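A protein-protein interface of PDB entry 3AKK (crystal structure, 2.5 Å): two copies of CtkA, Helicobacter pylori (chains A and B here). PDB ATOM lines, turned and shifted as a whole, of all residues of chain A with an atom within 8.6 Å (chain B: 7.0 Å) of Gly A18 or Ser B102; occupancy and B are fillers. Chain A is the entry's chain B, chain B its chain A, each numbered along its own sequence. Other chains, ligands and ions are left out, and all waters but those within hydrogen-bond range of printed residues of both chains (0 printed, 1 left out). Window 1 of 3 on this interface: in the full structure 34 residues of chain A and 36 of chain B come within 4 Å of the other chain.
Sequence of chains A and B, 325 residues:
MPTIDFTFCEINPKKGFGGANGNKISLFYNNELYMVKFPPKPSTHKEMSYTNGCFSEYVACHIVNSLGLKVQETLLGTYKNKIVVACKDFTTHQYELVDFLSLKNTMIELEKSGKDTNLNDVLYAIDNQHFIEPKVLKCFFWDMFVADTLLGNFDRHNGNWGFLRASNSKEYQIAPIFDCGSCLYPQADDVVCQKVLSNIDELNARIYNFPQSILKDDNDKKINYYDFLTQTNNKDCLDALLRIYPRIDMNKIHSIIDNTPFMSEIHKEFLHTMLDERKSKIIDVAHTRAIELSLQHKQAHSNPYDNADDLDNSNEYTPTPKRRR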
ATOM      1  N   LYS A  15       2.566  16.228  15.287  1.00  0.00           N
ATOM      2  CA  LYS A  15       3.868  16.804  14.998  1.00  0.00           C
ATOM      3  C   LYS A  15       4.154  16.856  13.499  1.00  0.00           C
ATOM      4  O   LYS A  15       3.807  15.950  12.747  1.00  0.00           O
ATOM      5  CB  LYS A  15       4.980  16.061  15.757  1.00  0.00           C
ATOM      6  CG  LYS A  15       6.318  16.781  15.722  1.00  0.00           C
ATOM      7  CD  LYS A  15       7.008  16.769  17.067  1.00  0.00           C
ATOM      8  CE  LYS A  15       8.413  17.347  16.968  1.00  0.00           C
ATOM      9  NZ  LYS A  15       9.286  17.027  18.164  1.00  0.00           N
ATOM     10  N   GLY A  16       4.779  17.941  13.075  1.00  0.00           N
ATOM     11  CA  GLY A  16       5.274  18.055  11.723  1.00  0.00           C
ATOM     12  C   GLY A  16       6.676  18.616  11.788  1.00  0.00           C
ATOM     13  O   GLY A  16       7.199  18.908  12.867  1.00  0.00           O
ATOM     14  N   PHE A  17       7.279  18.786  10.625  1.00  0.00           N
ATOM     15  CA  PHE A  17       8.652  19.253  10.515  1.00  0.00           C
ATOM     16  C   PHE A  17       8.731  20.154   9.298  1.00  0.00           C
ATOM     17  O   PHE A  17       7.946  20.026   8.354  1.00  0.00           O
ATOM     18  CB  PHE A  17       9.612  18.047  10.370  1.00  0.00           C
ATOM     19  CG  PHE A  17       9.544  17.101  11.531  1.00  0.00           C
ATOM     20  CD1 PHE A  17      10.359  17.285  12.633  1.00  0.00           C
ATOM     21  CD2 PHE A  17       8.607  16.067  11.551  1.00  0.00           C
ATOM     22  CE1 PHE A  17      10.259  16.452  13.731  1.00  0.00           C
ATOM     23  CE2 PHE A  17       8.504  15.226  12.635  1.00  0.00           C
ATOM     24  CZ  PHE A  17       9.333  15.417  13.731  1.00  0.00           C
ATOM     25  N   GLY A  18       9.681  21.069   9.313  1.00  0.00           N
ATOM     26  CA  GLY A  18       9.823  21.994   8.208  1.00  0.00           C
ATOM     27  C   GLY A  18      10.605  21.387   7.071  1.00  0.00           C
ATOM     28  O   GLY A  18      10.549  20.167   6.843  1.00  0.00           O
ATOM     29  N   GLY A  19      11.339  22.251   6.369  1.00  0.00           N
ATOM     30  CA  GLY A  19      12.125  21.878   5.205  1.00  0.00           C
ATOM     31  C   GLY A  19      11.307  21.606   3.951  1.00  0.00           C
ATOM     32  O   GLY A  19      10.139  21.222   4.029  1.00  0.00           O
ATOM     33  N   ALA A  20      11.940  21.776   2.793  1.00  0.00           N
ATOM     34  CA  ALA A  20      11.280  21.585   1.506  1.00  0.00           C
ATOM     35  C   ALA A  20      11.722  20.309   0.795  1.00  0.00           C
ATOM     36  O   ALA A  20      11.170  19.949  -0.243  1.00  0.00           O
ATOM     37  CB  ALA A  20      11.532  22.778   0.611  1.00  0.00           C
ATOM     38  N   ASN A  21      12.713  19.620   1.338  1.00  0.00           N
ATOM     39  CA  ASN A  21      13.351  18.550   0.580  1.00  0.00           C
ATOM     40  C   ASN A  21      12.645  17.210   0.592  1.00  0.00           C
ATOM     41  O   ASN A  21      13.188  16.230   0.086  1.00  0.00           O
ATOM     42  CB  ASN A  21      14.818  18.383   0.987  1.00  0.00           C
ATOM     43  CG  ASN A  21      15.714  19.453   0.384  1.00  0.00           C
ATOM     44  OD1 ASN A  21      15.276  20.265  -0.440  1.00  0.00           O
ATOM     45  ND2 ASN A  21      16.982  19.454   0.789  1.00  0.00           N
ATOM     46  N   GLY A  22      11.445  17.163   1.152  1.00  0.00           N
ATOM     47  CA  GLY A  22      10.627  15.963   1.102  1.00  0.00           C
ATOM     48  C   GLY A  22       9.578  15.992   2.189  1.00  0.00           C
ATOM     49  O   GLY A  22       9.495  16.971   2.943  1.00  0.00           O
ATOM     50  N   ASN A  23       8.771  14.938   2.275  1.00  0.00           N
ATOM     51  CA  ASN A  23       7.790  14.825   3.346  1.00  0.00           C
ATOM     52  C   ASN A  23       8.414  14.275   4.626  1.00  0.00           C
ATOM     53  O   ASN A  23       9.376  13.520   4.558  1.00  0.00           O
ATOM     54  CB  ASN A  23       6.622  13.941   2.909  1.00  0.00           C
ATOM     55  CG  ASN A  23       5.791  14.573   1.787  1.00  0.00           C
ATOM     56  OD1 ASN A  23       5.158  13.878   0.997  1.00  0.00           O
ATOM     57  ND2 ASN A  23       5.806  15.893   1.714  1.00  0.00           N
ATOM     58  N   LYS A  24       7.882  14.666   5.789  1.00  0.00           N
ATOM     59  CA  LYS A  24       8.268  14.068   7.074  1.00  0.00           C
ATOM     60  C   LYS A  24       7.034  13.676   7.879  1.00  0.00           C
ATOM     61  O   LYS A  24       6.045  14.397   7.867  1.00  0.00           O
ATOM     62  CB  LYS A  24       9.071  15.059   7.912  1.00  0.00           C
ATOM     63  CG  LYS A  24      10.384  15.513   7.305  1.00  0.00           C
ATOM     64  CD  LYS A  24      10.211  16.577   6.235  1.00  0.00           C
ATOM     65  CE  LYS A  24      11.530  16.786   5.521  1.00  0.00           C
ATOM     66  NZ  LYS A  24      11.562  18.029   4.746  1.00  0.00           N
ATOM     67  N   ILE A  25       7.084  12.555   8.589  1.00  0.00           N
ATOM     68  CA  ILE A  25       6.081  12.282   9.616  1.00  0.00           C
ATOM     69  C   ILE A  25       6.750  12.029  10.963  1.00  0.00           C
ATOM     70  O   ILE A  25       7.925  11.652  11.026  1.00  0.00           O
ATOM     71  CB  ILE A  25       5.154  11.091   9.263  1.00  0.00           C
ATOM     72  CG1 ILE A  25       5.959   9.807   9.098  1.00  0.00           C
ATOM     73  CG2 ILE A  25       4.397  11.359   7.981  1.00  0.00           C
ATOM     74  CD1 ILE A  25       5.127   8.629   8.597  1.00  0.00           C
ATOM     75  N   SER A  26       6.001  12.267  12.036  1.00  0.00           N
ATOM     76  CA  SER A  26       6.410  11.864  13.367  1.00  0.00           C
ATOM     77  C   SER A  26       5.869  10.475  13.671  1.00  0.00           C
ATOM     78  O   SER A  26       4.654  10.243  13.577  1.00  0.00           O
ATOM     79  CB  SER A  26       5.858  12.820  14.411  1.00  0.00           C
ATOM     80  OG  SER A  26       6.323  12.466  15.697  1.00  0.00           O
ATOM     81  N   MET A  35      11.779  11.491  13.573  1.00  0.00           N
ATOM     82  CA  MET A  35      11.389  12.215  12.366  1.00  0.00           C
ATOM     83  C   MET A  35      11.732  11.372  11.160  1.00  0.00           C
ATOM     84  O   MET A  35      12.894  11.222  10.813  1.00  0.00           O
ATOM     85  CB  MET A  35      12.109  13.548  12.249  1.00  0.00           C
ATOM     86  CG  MET A  35      11.670  14.384  11.023  1.00  0.00           C
ATOM     87  SD  MET A  35      12.885  15.673  10.622  1.00  0.00           S
ATOM     88  CE  MET A  35      14.368  14.704  10.340  1.00  0.00           C
ATOM     89  N   LYS A  37      12.052  10.952   7.391  1.00  0.00           N
ATOM     90  CA  LYS A  37      12.129  11.707   6.149  1.00  0.00           C
ATOM     91  C   LYS A  37      11.923  10.824   4.934  1.00  0.00           C
ATOM     92  O   LYS A  37      12.646   9.856   4.730  1.00  0.00           O
ATOM     93  CB  LYS A  37      13.469  12.431   6.034  1.00  0.00           C
ATOM     94  CG  LYS A  37      13.894  13.119   7.314  1.00  0.00           C
ATOM     95  CD  LYS A  37      14.801  14.283   7.004  1.00  0.00           C
ATOM     96  CE  LYS A  37      15.928  13.893   6.102  1.00  0.00           C
ATOM     97  NZ  LYS A  37      16.865  15.031   5.940  1.00  0.00           N
ATOM     98  N   LEU A  97      13.869  23.719  18.734  1.00  0.00           N
ATOM     99  CA  LEU A  97      15.022  23.951  17.876  1.00  0.00           C
ATOM    100  C   LEU A  97      15.011  25.331  17.243  1.00  0.00           C
ATOM    101  O   LEU A  97      14.071  25.701  16.557  1.00  0.00           O
ATOM    102  CB  LEU A  97      15.084  22.893  16.783  1.00  0.00           C
ATOM    103  CG  LEU A  97      16.113  23.087  15.668  1.00  0.00           C
ATOM    104  CD1 LEU A  97      17.540  22.886  16.157  1.00  0.00           C
ATOM    105  CD2 LEU A  97      15.803  22.135  14.553  1.00  0.00           C
ATOM    106  N   ASP A 179      20.466  17.135   9.400  1.00  0.00           N
ATOM    107  CA  ASP A 179      20.451  17.217   7.958  1.00  0.00           C
ATOM    108  C   ASP A 179      21.843  17.177   7.319  1.00  0.00           C
ATOM    109  O   ASP A 179      22.384  18.211   6.902  1.00  0.00           O
ATOM    110  CB  ASP A 179      19.671  18.435   7.477  1.00  0.00           C
ATOM    111  CG  ASP A 179      19.449  18.409   5.980  1.00  0.00           C
ATOM    112  OD1 ASP A 179      20.026  17.522   5.319  1.00  0.00           O
ATOM    113  OD2 ASP A 179      18.711  19.258   5.462  1.00  0.00           O
ATOM    114  N   LEU B  97       5.402  28.451  17.335  1.00  0.00           N
ATOM    115  CA  LEU B  97       4.743  28.573  16.054  1.00  0.00           C
ATOM    116  C   LEU B  97       5.137  27.369  15.203  1.00  0.00           C
ATOM    117  O   LEU B  97       6.320  27.118  14.957  1.00  0.00           O
ATOM    118  CB  LEU B  97       5.133  29.882  15.369  1.00  0.00           C
ATOM    119  CG  LEU B  97       4.640  30.032  13.930  1.00  0.00           C
ATOM    120  CD1 LEU B  97       3.121  30.065  13.865  1.00  0.00           C
ATOM    121  CD2 LEU B  97       5.235  31.277  13.326  1.00  0.00           C
ATOM    122  N   VAL B  98       4.134  26.607  14.790  1.00  0.00           N
ATOM    123  CA  VAL B  98       4.320  25.521  13.848  1.00  0.00           C
ATOM    124  C   VAL B  98       3.593  25.916  12.577  1.00  0.00           C
ATOM    125  O   VAL B  98       2.368  25.957  12.562  1.00  0.00           O
ATOM    126  CB  VAL B  98       3.674  24.229  14.367  1.00  0.00           C
ATOM    127  CG1 VAL B  98       3.815  23.114  13.332  1.00  0.00           C
ATOM    128  CG2 VAL B  98       4.267  23.844  15.701  1.00  0.00           C
ATOM    129  N   ASP B  99       4.337  26.213  11.515  1.00  0.00           N
ATOM    130  CA  ASP B  99       3.716  26.661  10.275  1.00  0.00           C
ATOM    131  C   ASP B  99       2.978  25.554   9.505  1.00  0.00           C
ATOM    132  O   ASP B  99       3.224  24.377   9.707  1.00  0.00           O
ATOM    133  CB  ASP B  99       4.711  27.416   9.391  1.00  0.00           C
ATOM    134  CG  ASP B  99       5.838  26.538   8.864  1.00  0.00           C
ATOM    135  OD1 ASP B  99       5.713  25.290   8.882  1.00  0.00           O
ATOM    136  OD2 ASP B  99       6.857  27.110   8.412  1.00  0.00           O
ATOM    137  N   PHE B 100       2.054  25.949   8.634  1.00  0.00           N
ATOM    138  CA  PHE B 100       1.276  24.992   7.853  1.00  0.00           C
ATOM    139  C   PHE B 100       2.191  24.135   6.982  1.00  0.00           C
ATOM    140  O   PHE B 100       1.969  22.941   6.835  1.00  0.00           O
ATOM    141  CB  PHE B 100       0.235  25.717   7.006  1.00  0.00           C
ATOM    142  CG  PHE B 100      -0.573  24.818   6.136  1.00  0.00           C
ATOM    143  CD1 PHE B 100      -1.483  23.945   6.677  1.00  0.00           C
ATOM    144  CD2 PHE B 100      -0.447  24.868   4.766  1.00  0.00           C
ATOM    145  CE1 PHE B 100      -2.246  23.123   5.869  1.00  0.00           C
ATOM    146  CE2 PHE B 100      -1.205  24.045   3.952  1.00  0.00           C
ATOM    147  CZ  PHE B 100      -2.102  23.172   4.506  1.00  0.00           C
ATOM    148  N   LEU B 101       3.235  24.739   6.435  1.00  0.00           N
ATOM    149  CA  LEU B 101       4.244  23.971   5.719  1.00  0.00           C
ATOM    150  C   LEU B 101       4.627  22.690   6.472  1.00  0.00           C
ATOM    151  O   LEU B 101       4.600  21.605   5.896  1.00  0.00           O
ATOM    152  CB  LEU B 101       5.473  24.827   5.438  1.00  0.00           C
ATOM    153  CG  LEU B 101       6.569  24.270   4.527  1.00  0.00           C
ATOM    154  CD1 LEU B 101       7.292  25.409   3.801  1.00  0.00           C
ATOM    155  CD2 LEU B 101       7.542  23.444   5.344  1.00  0.00           C
ATOM    156  N   SER B 102       4.966  22.812   7.757  1.00  0.00           N
ATOM    157  CA  SER B 102       5.307  21.631   8.546  1.00  0.00           C
ATOM    158  C   SER B 102       4.152  20.646   8.543  1.00  0.00           C
ATOM    159  O   SER B 102       4.329  19.451   8.289  1.00  0.00           O
ATOM    160  CB  SER B 102       5.659  21.994   9.988  1.00  0.00           C
ATOM    161  OG  SER B 102       6.893  22.684  10.046  1.00  0.00           O
ATOM    162  N   LEU B 103       2.963  21.158   8.830  1.00  0.00           N
ATOM    163  CA  LEU B 103       1.800  20.315   8.876  1.00  0.00           C
ATOM    164  C   LEU B 103       1.592  19.680   7.497  1.00  0.00           C
ATOM    165  O   LEU B 103       1.291  18.493   7.402  1.00  0.00           O
ATOM    166  CB  LEU B 103       0.576  21.117   9.340  1.00  0.00           C
ATOM    167  CG  LEU B 103      -0.746  20.356   9.481  1.00  0.00           C
ATOM    168  CD1 LEU B 103      -1.445  20.201   8.137  1.00  0.00           C
ATOM    169  CD2 LEU B 103      -0.508  18.997  10.120  1.00  0.00           C
ATOM    170  N   LYS B 104       1.776  20.453   6.429  1.00  0.00           N
ATOM    171  CA  LYS B 104       1.538  19.923   5.092  1.00  0.00           C
ATOM    172  C   LYS B 104       2.576  18.859   4.718  1.00  0.00           C
ATOM    173  O   LYS B 104       2.281  17.922   3.961  1.00  0.00           O
ATOM    174  CB  LYS B 104       1.478  21.035   4.036  1.00  0.00           C
ATOM    175  CG  LYS B 104       1.097  20.548   2.638  1.00  0.00           C
ATOM    176  CD  LYS B 104       0.935  21.710   1.662  1.00  0.00           C
ATOM    177  CE  LYS B 104       0.502  21.262   0.253  1.00  0.00           C
ATOM    178  NZ  LYS B 104       1.537  20.394  -0.436  1.00  0.00           N
ATOM    179  N   ASN B 105       3.784  19.000   5.260  1.00  0.00           N
ATOM    180  CA  ASN B 105       4.828  18.001   5.078  1.00  0.00           C
ATOM    181  C   ASN B 105       4.404  16.630   5.566  1.00  0.00           C
ATOM    182  O   ASN B 105       4.915  15.623   5.099  1.00  0.00           O
ATOM    183  CB  ASN B 105       6.116  18.426   5.766  1.00  0.00           C
ATOM    184  CG  ASN B 105       7.056  19.123   4.828  1.00  0.00           C
ATOM    185  OD1 ASN B 105       6.861  19.084   3.616  1.00  0.00           O
ATOM    186  ND2 ASN B 105       8.075  19.777   5.370  1.00  0.00           N
ATOM    187  N   THR B 106       3.455  16.580   6.494  1.00  0.00           N
ATOM    188  CA  THR B 106       2.981  15.282   6.972  1.00  0.00           C
ATOM    189  C   THR B 106       2.117  14.488   5.981  1.00  0.00           C
ATOM    190  O   THR B 106       1.975  13.282   6.132  1.00  0.00           O
ATOM    191  CB  THR B 106       2.242  15.385   8.324  1.00  0.00           C
ATOM    192  OG1 THR B 106       0.905  15.863   8.111  1.00  0.00           O
ATOM    193  CG2 THR B 106       2.992  16.305   9.268  1.00  0.00           C
ATOM    194  N   MET B 107       1.553  15.149   4.976  1.00  0.00           N
ATOM    195  CA  MET B 107       0.655  14.477   4.019  1.00  0.00           C
ATOM    196  C   MET B 107       1.412  13.644   2.985  1.00  0.00           C
ATOM    197  O   MET B 107       1.321  13.918   1.784  1.00  0.00           O
ATOM    198  CB  MET B 107      -0.253  15.486   3.296  1.00  0.00           C
ATOM    199  CG  MET B 107      -1.052  16.407   4.212  1.00  0.00           C
ATOM    200  SD  MET B 107      -2.061  15.448   5.334  1.00  0.00           S
ATOM    201  CE  MET B 107      -2.678  16.708   6.455  1.00  0.00           C
ATOM    202  N   GLY B 114       5.655  19.864   1.089  1.00  0.00           N
ATOM    203  CA  GLY B 114       4.801  20.705   1.905  1.00  0.00           C
ATOM    204  C   GLY B 114       4.931  22.180   1.578  1.00  0.00           C
ATOM    205  O   GLY B 114       4.128  22.993   2.029  1.00  0.00           O
ATOM    206  N   PHE B 131      -4.296  18.682  13.946  1.00  0.00           N
ATOM    207  CA  PHE B 131      -3.945  19.764  14.864  1.00  0.00           C
ATOM    208  C   PHE B 131      -5.203  20.449  15.396  1.00  0.00           C
ATOM    209  O   PHE B 131      -5.276  20.878  16.546  1.00  0.00           O
ATOM    210  CB  PHE B 131      -3.094  20.802  14.135  1.00  0.00           C
ATOM    211  CG  PHE B 131      -1.679  20.363  13.869  1.00  0.00           C
ATOM    212  CD1 PHE B 131      -0.694  21.299  13.572  1.00  0.00           C
ATOM    213  CD2 PHE B 131      -1.327  19.029  13.934  1.00  0.00           C
ATOM    214  CE1 PHE B 131       0.601  20.916  13.337  1.00  0.00           C
ATOM    215  CE2 PHE B 131      -0.028  18.640  13.709  1.00  0.00           C
ATOM    216  CZ  PHE B 131       0.938  19.590  13.410  1.00  0.00           C
ATOM    217  N   ASN B 158       3.061  28.495   2.399  1.00  0.00           N
ATOM    218  CA  ASN B 158       2.669  27.589   3.465  1.00  0.00           C
ATOM    219  C   ASN B 158       3.384  27.834   4.791  1.00  0.00           C
ATOM    220  O   ASN B 158       3.001  27.277   5.830  1.00  0.00           O
ATOM    221  CB  ASN B 158       2.813  26.142   3.001  1.00  0.00           C
ATOM    222  CG  ASN B 158       1.827  25.797   1.915  1.00  0.00           C
ATOM    223  OD1 ASN B 158       0.705  26.303   1.919  1.00  0.00           O
ATOM    224  ND2 ASN B 158       2.231  24.949   0.972  1.00  0.00           N
ATOM    225  N   GLY B 159       4.411  28.676   4.756  1.00  0.00           N
ATOM    226  CA  GLY B 159       5.081  29.096   5.978  1.00  0.00           C
ATOM    227  C   GLY B 159       4.669  30.495   6.455  1.00  0.00           C
ATOM    228  O   GLY B 159       5.201  31.011   7.443  1.00  0.00           O
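O of Gly A19 is in hydrogen-bond range of ND2 of Asn B105 (2.9 Å). The side-chain hydroxyl of Ser B102 sits close to the backbone carbonyl oxygen of Phe A17. The side-chain amide nitrogen (ND2) of Asn B105 sits at hydrogen-bond distance from the backbone carbonyl oxygen (O) of Phe A17. ND2 of Asn B105 sits at hydrogen-bond distance from O of Gly A18 (2.9 Å). The backbone carbonyl oxygen (O) of Gly A22 sits close to the side-chain amide oxygen (OD1) of Asn B105. The backbone NH (N) of Lys A24 lies within hydrogen-bond range of the backbone carbonyl oxygen (O) of Asn B105. N of Gly A18 lies within hydrogen-bond range of OG of Ser B102.
O of Asn B158 sits at hydrogen-bond distance from N of Leu B101 (2.6 Å). The side-chain amide oxygen (OD1) of Asn B105 is in hydrogen-bond range of the backbone NH (N) of Gly B114, at 2.9 Å. OG1 of Thr B106 sits at hydrogen-bond distance from O of Leu B103, at 2.8 Å. NZ of Lys A24 lies within hydrogen-bond range of O of Gly A18 (3.2 Å). The backbone carbonyl oxygen (O) of Gly A22 lies within hydrogen-bond range of the side-chain amino group (NZ) of Lys A24 (2.9 Å). The side-chain carboxylate (OD1) of Asp B99 is in hydrogen-bond range of the backbone NH (N) of Ser B102, at 2.8 Å.
Among the printed residues, pairs that only touch across the chains: Lys A15 with Thr B106 (3.6 Å), Lys A15 with Phe B131 (3.9 Å), Gly A16 with Ser B102 (3.8 Å), Gly A16 with Thr B106 (3.8 Å), Gly A18 with Leu B101 (3.9 Å), Gly A19 with Leu B101 (3.7 Å), Asn A23 with Asn B105 (3.2 Å), Asn A23 with Met B107 (3.9 Å), Lys A24 with Thr B106 (3.3 Å) and Ile A25 with Thr B106 (3.6 Å).
Of the printed residues of chain B, Gly A22 touches Asn B105 (3.4 Å). Val B98 touches none of the printed residues of chain A. Of chain A, only Gly A16 (3.8 Å), Phe A17 (3.1 Å) and Gly A18 (3.3 Å) come within 4 Å of Ser B102. Printed residues of chain A within 4 Å of Met B107: Asn A23 (3.9 Å). Printed residues of chain A within 4 Å of Phe B131: Lys A15 (3.9 Å). The nearest residue of chain B that does not touch Gly A18 is Asp B99 (5.3 Å).
Printed residues of chain A that touch a printed residue of chain B: Lys A15, Gly A16, Phe A17, Gly A18, Gly A19, Gly A22, Asn A23, Lys A24 and Ile A25. Hydrophobic or aromatic side chains of chain A within 4 Å of the printed part of chain B: Ile A25. Along chain A the printed residues that touch a printed residue of chain B span positions 15 to 25. Hydrophobic or aromatic side chains of chain B that line the printed part of chain A: Leu B101 and Phe B131. Among the printed residues, 17 pairs touch across the chains.
1 position is printed for both chains.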
